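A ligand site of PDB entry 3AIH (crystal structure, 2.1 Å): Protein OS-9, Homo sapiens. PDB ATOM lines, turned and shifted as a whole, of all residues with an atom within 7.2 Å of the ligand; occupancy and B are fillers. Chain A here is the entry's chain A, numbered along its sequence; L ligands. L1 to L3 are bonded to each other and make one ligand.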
ATOM      1  N   LYS A  10     -12.485  12.593 -16.799  1.00  0.00           N
ATOM      2  CA  LYS A  10     -12.844  11.238 -16.328  1.00  0.00           C
ATOM      3  C   LYS A  10     -12.883  11.193 -14.770  1.00  0.00           C
ATOM      4  O   LYS A  10     -11.833  11.328 -14.111  1.00  0.00           O
ATOM      5  CB  LYS A  10     -11.836  10.215 -16.899  1.00  0.00           C
ATOM      6  CG  LYS A  10     -11.883   8.808 -16.283  1.00  0.00           C
ATOM      7  CD  LYS A  10     -10.553   8.030 -16.529  1.00  0.00           C
ATOM      8  CE  LYS A  10     -10.606   6.632 -15.916  1.00  0.00           C
ATOM      9  NZ  LYS A  10      -9.620   5.647 -16.476  1.00  0.00           N
ATOM     10  N   ASP A  11     -14.097  11.012 -14.200  1.00  0.00           N
ATOM     11  CA  ASP A  11     -14.361  11.183 -12.749  1.00  0.00           C
ATOM     12  C   ASP A  11     -13.753  12.484 -12.201  1.00  0.00           C
ATOM     13  O   ASP A  11     -14.190  13.588 -12.559  1.00  0.00           O
ATOM     14  CB  ASP A  11     -13.844   9.994 -11.906  1.00  0.00           C
ATOM     15  CG  ASP A  11     -14.198   8.643 -12.489  1.00  0.00           C
ATOM     16  OD1 ASP A  11     -15.412   8.328 -12.636  1.00  0.00           O
ATOM     17  OD2 ASP A  11     -13.245   7.877 -12.802  1.00  0.00           O
ATOM     18  N   TRP A  12     -12.760  12.357 -11.337  1.00  0.00           N
ATOM     19  CA  TRP A  12     -12.199  13.480 -10.646  1.00  0.00           C
ATOM     20  C   TRP A  12     -11.306  14.363 -11.528  1.00  0.00           C
ATOM     21  O   TRP A  12     -11.267  15.593 -11.389  1.00  0.00           O
ATOM     22  CB  TRP A  12     -11.350  12.986  -9.466  1.00  0.00           C
ATOM     23  CG  TRP A  12     -11.000  14.093  -8.571  1.00  0.00           C
ATOM     24  CD1 TRP A  12      -9.780  14.725  -8.439  1.00  0.00           C
ATOM     25  CD2 TRP A  12     -11.879  14.707  -7.663  1.00  0.00           C
ATOM     26  NE1 TRP A  12      -9.873  15.721  -7.488  1.00  0.00           N
ATOM     27  CE2 TRP A  12     -11.161  15.732  -7.013  1.00  0.00           C
ATOM     28  CE3 TRP A  12     -13.234  14.514  -7.350  1.00  0.00           C
ATOM     29  CZ2 TRP A  12     -11.737  16.540  -6.052  1.00  0.00           C
ATOM     30  CZ3 TRP A  12     -13.805  15.330  -6.410  1.00  0.00           C
ATOM     31  CH2 TRP A  12     -13.064  16.316  -5.771  1.00  0.00           C
ATOM     32  N   TRP A  13     -10.576  13.712 -12.415  1.00  0.00           N
ATOM     33  CA  TRP A  13      -9.531  14.357 -13.150  1.00  0.00           C
ATOM     34  C   TRP A  13      -9.944  14.848 -14.537  1.00  0.00           C
ATOM     35  O   TRP A  13     -10.696  14.166 -15.269  1.00  0.00           O
ATOM     36  CB  TRP A  13      -8.335  13.417 -13.221  1.00  0.00           C
ATOM     37  CG  TRP A  13      -7.739  13.130 -11.858  1.00  0.00           C
ATOM     38  CD1 TRP A  13      -7.696  11.898 -11.179  1.00  0.00           C
ATOM     39  CD2 TRP A  13      -7.111  14.081 -10.961  1.00  0.00           C
ATOM     40  NE1 TRP A  13      -7.043  12.048  -9.973  1.00  0.00           N
ATOM     41  CE2 TRP A  13      -6.688  13.373  -9.810  1.00  0.00           C
ATOM     42  CE3 TRP A  13      -6.845  15.456 -11.040  1.00  0.00           C
ATOM     43  CZ2 TRP A  13      -6.035  13.995  -8.734  1.00  0.00           C
ATOM     44  CZ3 TRP A  13      -6.145  16.070  -9.961  1.00  0.00           C
ATOM     45  CH2 TRP A  13      -5.758  15.334  -8.830  1.00  0.00           C
ATOM     46  N   TYR A  15      -8.047  15.990 -18.056  1.00  0.00           N
ATOM     47  CA  TYR A  15      -6.772  15.737 -18.689  1.00  0.00           C
ATOM     48  C   TYR A  15      -6.589  16.741 -19.828  1.00  0.00           C
ATOM     49  O   TYR A  15      -7.488  16.927 -20.618  1.00  0.00           O
ATOM     50  CB  TYR A  15      -6.739  14.280 -19.212  1.00  0.00           C
ATOM     51  CG  TYR A  15      -6.726  13.290 -18.070  1.00  0.00           C
ATOM     52  CD1 TYR A  15      -5.555  12.956 -17.431  1.00  0.00           C
ATOM     53  CD2 TYR A  15      -7.909  12.713 -17.613  1.00  0.00           C
ATOM     54  CE1 TYR A  15      -5.550  12.051 -16.349  1.00  0.00           C
ATOM     55  CE2 TYR A  15      -7.908  11.838 -16.544  1.00  0.00           C
ATOM     56  CZ  TYR A  15      -6.735  11.526 -15.915  1.00  0.00           C
ATOM     57  OH  TYR A  15      -6.757  10.656 -14.858  1.00  0.00           O
ATOM     58  N   GLN A  25      -2.988  16.970 -15.599  1.00  0.00           N
ATOM     59  CA  GLN A  25      -4.121  16.345 -14.934  1.00  0.00           C
ATOM     60  C   GLN A  25      -4.520  17.258 -13.763  1.00  0.00           C
ATOM     61  O   GLN A  25      -3.666  17.623 -12.957  1.00  0.00           O
ATOM     62  CB  GLN A  25      -3.685  14.953 -14.409  1.00  0.00           C
ATOM     63  CG  GLN A  25      -4.691  14.204 -13.541  1.00  0.00           C
ATOM     64  CD  GLN A  25      -4.114  12.894 -12.961  1.00  0.00           C
ATOM     65  OE1 GLN A  25      -4.720  11.829 -13.120  1.00  0.00           O
ATOM     66  NE2 GLN A  25      -2.967  12.976 -12.274  1.00  0.00           N
ATOM     67  N   GLU A  36      -3.870  22.187  -7.113  1.00  0.00           N
ATOM     68  CA  GLU A  36      -2.688  21.621  -7.778  1.00  0.00           C
ATOM     69  C   GLU A  36      -2.977  21.172  -9.211  1.00  0.00           C
ATOM     70  O   GLU A  36      -3.994  20.523  -9.484  1.00  0.00           O
ATOM     71  CB  GLU A  36      -2.267  20.371  -6.975  1.00  0.00           C
ATOM     72  CG  GLU A  36      -3.447  19.728  -6.199  1.00  0.00           C
ATOM     73  CD  GLU A  36      -4.073  18.451  -6.825  1.00  0.00           C
ATOM     74  OE1 GLU A  36      -5.257  18.491  -7.293  1.00  0.00           O
ATOM     75  OE2 GLU A  36      -3.392  17.395  -6.755  1.00  0.00           O
ATOM     76  N   LEU A  38      -1.347  18.705 -11.931  1.00  0.00           N
ATOM     77  CA  LEU A  38      -0.282  17.679 -12.017  1.00  0.00           C
ATOM     78  C   LEU A  38       0.182  17.491 -13.450  1.00  0.00           C
ATOM     79  O   LEU A  38      -0.593  17.563 -14.379  1.00  0.00           O
ATOM     80  CB  LEU A  38      -0.759  16.346 -11.438  1.00  0.00           C
ATOM     81  CG  LEU A  38      -1.038  16.356  -9.930  1.00  0.00           C
ATOM     82  CD1 LEU A  38      -1.960  15.145  -9.556  1.00  0.00           C
ATOM     83  CD2 LEU A  38       0.271  16.387  -9.109  1.00  0.00           C
ATOM     84  N   LEU A  40       1.523  14.861 -15.964  1.00  0.00           N
ATOM     85  CA  LEU A  40       1.713  13.456 -16.367  1.00  0.00           C
ATOM     86  C   LEU A  40       3.091  13.295 -16.990  1.00  0.00           C
ATOM     87  O   LEU A  40       3.722  12.257 -16.878  1.00  0.00           O
ATOM     88  CB  LEU A  40       0.593  13.028 -17.307  1.00  0.00           C
ATOM     89  CG  LEU A  40      -0.659  12.419 -16.626  1.00  0.00           C
ATOM     90  CD1 LEU A  40      -1.055  13.077 -15.343  1.00  0.00           C
ATOM     91  CD2 LEU A  40      -1.854  12.169 -17.512  1.00  0.00           C
ATOM     92  N   LYS A  75       6.263  14.187  -9.245  1.00  0.00           N
ATOM     93  CA  LYS A  75       6.607  13.063  -8.358  1.00  0.00           C
ATOM     94  C   LYS A  75       5.377  12.332  -7.871  1.00  0.00           C
ATOM     95  O   LYS A  75       4.381  12.945  -7.458  1.00  0.00           O
ATOM     96  CB  LYS A  75       7.435  13.554  -7.155  1.00  0.00           C
ATOM     97  CG  LYS A  75       8.689  14.294  -7.548  1.00  0.00           C
ATOM     98  CD  LYS A  75       9.873  13.373  -7.649  1.00  0.00           C
ATOM     99  CE  LYS A  75      10.541  13.211  -6.268  1.00  0.00           C
ATOM    100  NZ  LYS A  75      11.785  12.381  -6.357  1.00  0.00           N
ATOM    101  N   CYS A  76       5.448  11.005  -7.917  1.00  0.00           N
ATOM    102  CA  CYS A  76       4.378  10.134  -7.415  1.00  0.00           C
ATOM    103  C   CYS A  76       4.548   9.984  -5.905  1.00  0.00           C
ATOM    104  O   CYS A  76       5.661   9.759  -5.420  1.00  0.00           O
ATOM    105  CB  CYS A  76       4.505   8.738  -8.045  1.00  0.00           C
ATOM    106  SG  CYS A  76       3.012   7.733  -7.897  1.00  0.00           S
ATOM    107  N   ASP A  77       3.450  10.092  -5.155  1.00  0.00           N
ATOM    108  CA  ASP A  77       3.587  10.015  -3.695  1.00  0.00           C
ATOM    109  C   ASP A  77       3.716   8.552  -3.292  1.00  0.00           C
ATOM    110  O   ASP A  77       4.263   8.244  -2.239  1.00  0.00           O
ATOM    111  CB  ASP A  77       2.426  10.693  -2.950  1.00  0.00           C
ATOM    112  CG  ASP A  77       1.065  10.270  -3.485  1.00  0.00           C
ATOM    113  OD1 ASP A  77       1.026   9.529  -4.492  1.00  0.00           O
ATOM    114  OD2 ASP A  77       0.031  10.688  -2.924  1.00  0.00           O
ATOM    115  N   LEU A  78       3.268   7.658  -4.169  1.00  0.00           N
ATOM    116  CA  LEU A  78       3.336   6.243  -3.877  1.00  0.00           C
ATOM    117  C   LEU A  78       4.786   5.766  -3.840  1.00  0.00           C
ATOM    118  O   LEU A  78       5.133   4.944  -2.970  1.00  0.00           O
ATOM    119  CB  LEU A  78       2.465   5.444  -4.857  1.00  0.00           C
ATOM    120  CG  LEU A  78       0.959   5.388  -4.546  1.00  0.00           C
ATOM    121  CD1 LEU A  78       0.455   6.373  -3.441  1.00  0.00           C
ATOM    122  CD2 LEU A  78       0.151   5.558  -5.786  1.00  0.00           C
ATOM    123  N   ARG A  83       6.105  11.141 -12.686  1.00  0.00           N
ATOM    124  CA  ARG A  83       5.096  10.561 -13.556  1.00  0.00           C
ATOM    125  C   ARG A  83       5.675  10.434 -14.983  1.00  0.00           C
ATOM    126  O   ARG A  83       6.615  11.149 -15.377  1.00  0.00           O
ATOM    127  CB  ARG A  83       3.813  11.384 -13.487  1.00  0.00           C
ATOM    128  CG  ARG A  83       2.886  11.120 -12.252  1.00  0.00           C
ATOM    129  CD  ARG A  83       1.764  12.198 -12.163  1.00  0.00           C
ATOM    130  NE  ARG A  83       0.715  11.925 -11.175  1.00  0.00           N
ATOM    131  CZ  ARG A  83       0.875  12.051  -9.849  1.00  0.00           C
ATOM    132  NH1 ARG A  83       2.061  12.389  -9.352  1.00  0.00           N
ATOM    133  NH2 ARG A  83      -0.118  11.726  -9.014  1.00  0.00           N
ATOM    134  N   GLU A 107      -3.825   3.659 -16.715  1.00  0.00           N
ATOM    135  CA  GLU A 107      -2.685   3.805 -15.780  1.00  0.00           C
ATOM    136  C   GLU A 107      -2.204   2.456 -15.322  1.00  0.00           C
ATOM    137  O   GLU A 107      -2.573   2.021 -14.219  1.00  0.00           O
ATOM    138  CB  GLU A 107      -3.112   4.622 -14.546  1.00  0.00           C
ATOM    139  CG  GLU A 107      -1.931   5.041 -13.677  1.00  0.00           C
ATOM    140  CD  GLU A 107      -2.355   5.978 -12.496  1.00  0.00           C
ATOM    141  OE1 GLU A 107      -3.503   6.539 -12.517  1.00  0.00           O
ATOM    142  OE2 GLU A 107      -1.502   6.155 -11.591  1.00  0.00           O
ATOM    143  N   LEU A 109       0.660   1.102 -14.373  1.00  0.00           N
ATOM    144  CA  LEU A 109       1.422   1.094 -13.110  1.00  0.00           C
ATOM    145  C   LEU A 109       1.127   2.414 -12.468  1.00  0.00           C
ATOM    146  O   LEU A 109       0.959   3.418 -13.194  1.00  0.00           O
ATOM    147  CB  LEU A 109       2.948   1.004 -13.345  1.00  0.00           C
ATOM    148  CG  LEU A 109       3.536  -0.294 -13.918  1.00  0.00           C
ATOM    149  CD1 LEU A 109       3.280  -0.334 -15.398  1.00  0.00           C
ATOM    150  CD2 LEU A 109       5.027  -0.398 -13.638  1.00  0.00           C
ATOM    151  N   SER A 110       1.115   2.463 -11.122  1.00  0.00           N
ATOM    152  CA  SER A 110       0.999   3.743 -10.419  1.00  0.00           C
ATOM    153  C   SER A 110       1.842   4.833 -11.053  1.00  0.00           C
ATOM    154  O   SER A 110       3.048   4.695 -11.120  1.00  0.00           O
ATOM    155  CB  SER A 110       1.401   3.632  -8.931  1.00  0.00           C
ATOM    156  OG  SER A 110       0.344   2.987  -8.248  1.00  0.00           O
ATOM    157  N   CYS A 111       1.194   5.916 -11.480  1.00  0.00           N
ATOM    158  CA  CYS A 111       1.906   7.088 -12.024  1.00  0.00           C
ATOM    159  C   CYS A 111       2.639   6.861 -13.382  1.00  0.00           C
ATOM    160  O   CYS A 111       3.509   7.630 -13.778  1.00  0.00           O
ATOM    161  CB  CYS A 111       2.834   7.706 -10.959  1.00  0.00           C
ATOM    162  SG  CYS A 111       1.880   8.413  -9.545  1.00  0.00           S
ATOM    163  N   SER A 112       2.240   5.792 -14.065  1.00  0.00           N
ATOM    164  CA  SER A 112       2.667   5.548 -15.451  1.00  0.00           C
ATOM    165  C   SER A 112       1.415   5.438 -16.287  1.00  0.00           C
ATOM    166  O   SER A 112       0.570   4.584 -16.015  1.00  0.00           O
ATOM    167  CB  SER A 112       3.495   4.272 -15.554  1.00  0.00           C
ATOM    168  OG  SER A 112       4.578   4.363 -14.639  1.00  0.00           O
ATOM    169  N   TYR A 113       1.301   6.269 -17.315  1.00  0.00           N
ATOM    170  CA  TYR A 113       0.050   6.392 -18.034  1.00  0.00           C
ATOM    171  C   TYR A 113       0.175   6.062 -19.482  1.00  0.00           C
ATOM    172  O   TYR A 113       1.241   6.292 -20.108  1.00  0.00           O
ATOM    173  CB  TYR A 113      -0.449   7.830 -17.956  1.00  0.00           C
ATOM    174  CG  TYR A 113      -0.605   8.311 -16.546  1.00  0.00           C
ATOM    175  CD1 TYR A 113      -1.854   8.296 -15.924  1.00  0.00           C
ATOM    176  CD2 TYR A 113       0.508   8.811 -15.825  1.00  0.00           C
ATOM    177  CE1 TYR A 113      -2.026   8.771 -14.579  1.00  0.00           C
ATOM    178  CE2 TYR A 113       0.364   9.276 -14.488  1.00  0.00           C
ATOM    179  CZ  TYR A 113      -0.907   9.252 -13.890  1.00  0.00           C
ATOM    180  OH  TYR A 113      -1.043   9.733 -12.594  1.00  0.00           O
HETATM  181  O1  LIG L   1      -8.924  11.888  -5.376  1.00  0.00           O
HETATM  182  C1  LG2 L   2      -8.576  11.434  -6.694  1.00  0.00           C
HETATM  183  C2  LG2 L   2      -9.055  10.006  -6.936  1.00  0.00           C
HETATM  184  C3  LG2 L   2      -8.163   9.013  -6.172  1.00  0.00           C
HETATM  185  C4  LG2 L   2      -6.710   9.273  -6.430  1.00  0.00           C
HETATM  186  C5  LG2 L   2      -6.363  10.712  -6.089  1.00  0.00           C
HETATM  187  C6  LG2 L   2      -4.899  10.986  -6.363  1.00  0.00           C
HETATM  188  O1  LG2 L   2      -8.978   9.778  -8.317  1.00  0.00           O
HETATM  189  O2  LG2 L   2      -8.505   7.680  -6.498  1.00  0.00           O
HETATM  190  O3  LG2 L   2      -5.967   8.434  -5.619  1.00  0.00           O
HETATM  191  O4  LG2 L   2      -7.163  11.504  -6.931  1.00  0.00           O
HETATM  192  O5  LG2 L   2      -4.723  10.708  -7.749  1.00  0.00           O
HETATM  193  C1  LG3 L   3      -3.472  11.150  -8.262  1.00  0.00           C
HETATM  194  C2  LG3 L   3      -3.466  10.890  -9.796  1.00  0.00           C
HETATM  195  C3  LG3 L   3      -3.443   9.372 -10.109  1.00  0.00           C
HETATM  196  C4  LG3 L   3      -2.362   8.636  -9.331  1.00  0.00           C
HETATM  197  C5  LG3 L   3      -2.399   9.057  -7.846  1.00  0.00           C
HETATM  198  C6  LG3 L   3      -1.210   8.441  -7.132  1.00  0.00           C
HETATM  199  O1  LG3 L   3      -2.288  11.461 -10.335  1.00  0.00           O
HETATM  200  O2  LG3 L   3      -3.357   9.152 -11.520  1.00  0.00           O
HETATM  201  O3  LG3 L   3      -2.664   7.244  -9.465  1.00  0.00           O
HETATM  202  O4  LG3 L   3      -2.377  10.482  -7.680  1.00  0.00           O
HETATM  203  O5  LG3 L   3      -1.051   8.964  -5.824  1.00  0.00           O
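OE2 of Glu 107 is in hydrogen-bond range of O3 of LG3 L3, 2.7 Å away. NE1 of Trp 13 is in hydrogen-bond range of O4 of LG2 L2, at 3.1 Å. An oxygen (O2) of LG3 L3 is in hydrogen-bond range of the side-chain hydroxyl (OH) of Tyr 113, at 2.6 Å. An oxygen (O1) of LG3 L3 sits at hydrogen-bond distance from the side-chain amide nitrogen of Gln 25, 2.6 Å away. The guanidinium group (NH2) of Arg 83 lies within hydrogen-bond range of an oxygen (O1) of LG3 L3 (2.6 Å). O5 of LG3 L3 sits at hydrogen-bond distance from OD1 of Asp 77, at 2.5 Å.
SG of Cys 76 forms a disulfide with SG of Cys 111 (2.1 Å). The backbone carbonyl oxygen of Leu 38 lies within hydrogen-bond range of the backbone NH of Gln 25 (2.8 Å). OE2 of Glu 107 sits at hydrogen-bond distance from N of Cys 111 (2.7 Å). The side-chain sulfur of Cys 76 lies close to the backbone NH of Leu 78 (3.7 Å). NE of Arg 83 is in hydrogen-bond range of OH of Tyr 113 (3.1 Å). NH1 of Arg 83 sits at hydrogen-bond distance from O of Lys 75 (3.0 Å). OE1 of Gln 25 is in hydrogen-bond range of OH of Tyr 15 (2.9 Å).
CD1 of Trp 12 touches C1 of LG2 L2, at 3.9 Å. CD1 of Leu 38 touches O1 of LG3 L3, at 3.8 Å. CD2 of Leu 78 touches C6 of LG3 L3 (3.5 Å). SG of Cys 111 touches C6 of LG3 L3, 3.9 Å away. Hydrophobic or aromatic side chains within 4 Å of the ligand: Trp 12, Trp 13, Leu 38, Leu 78 and Tyr 113. Within 4 Å of the ligand: Trp 12, Trp 13, Gln 25, Leu 38, Asp 77, Leu 78, Arg 83, Glu 107, Cys 111 and Tyr 113.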
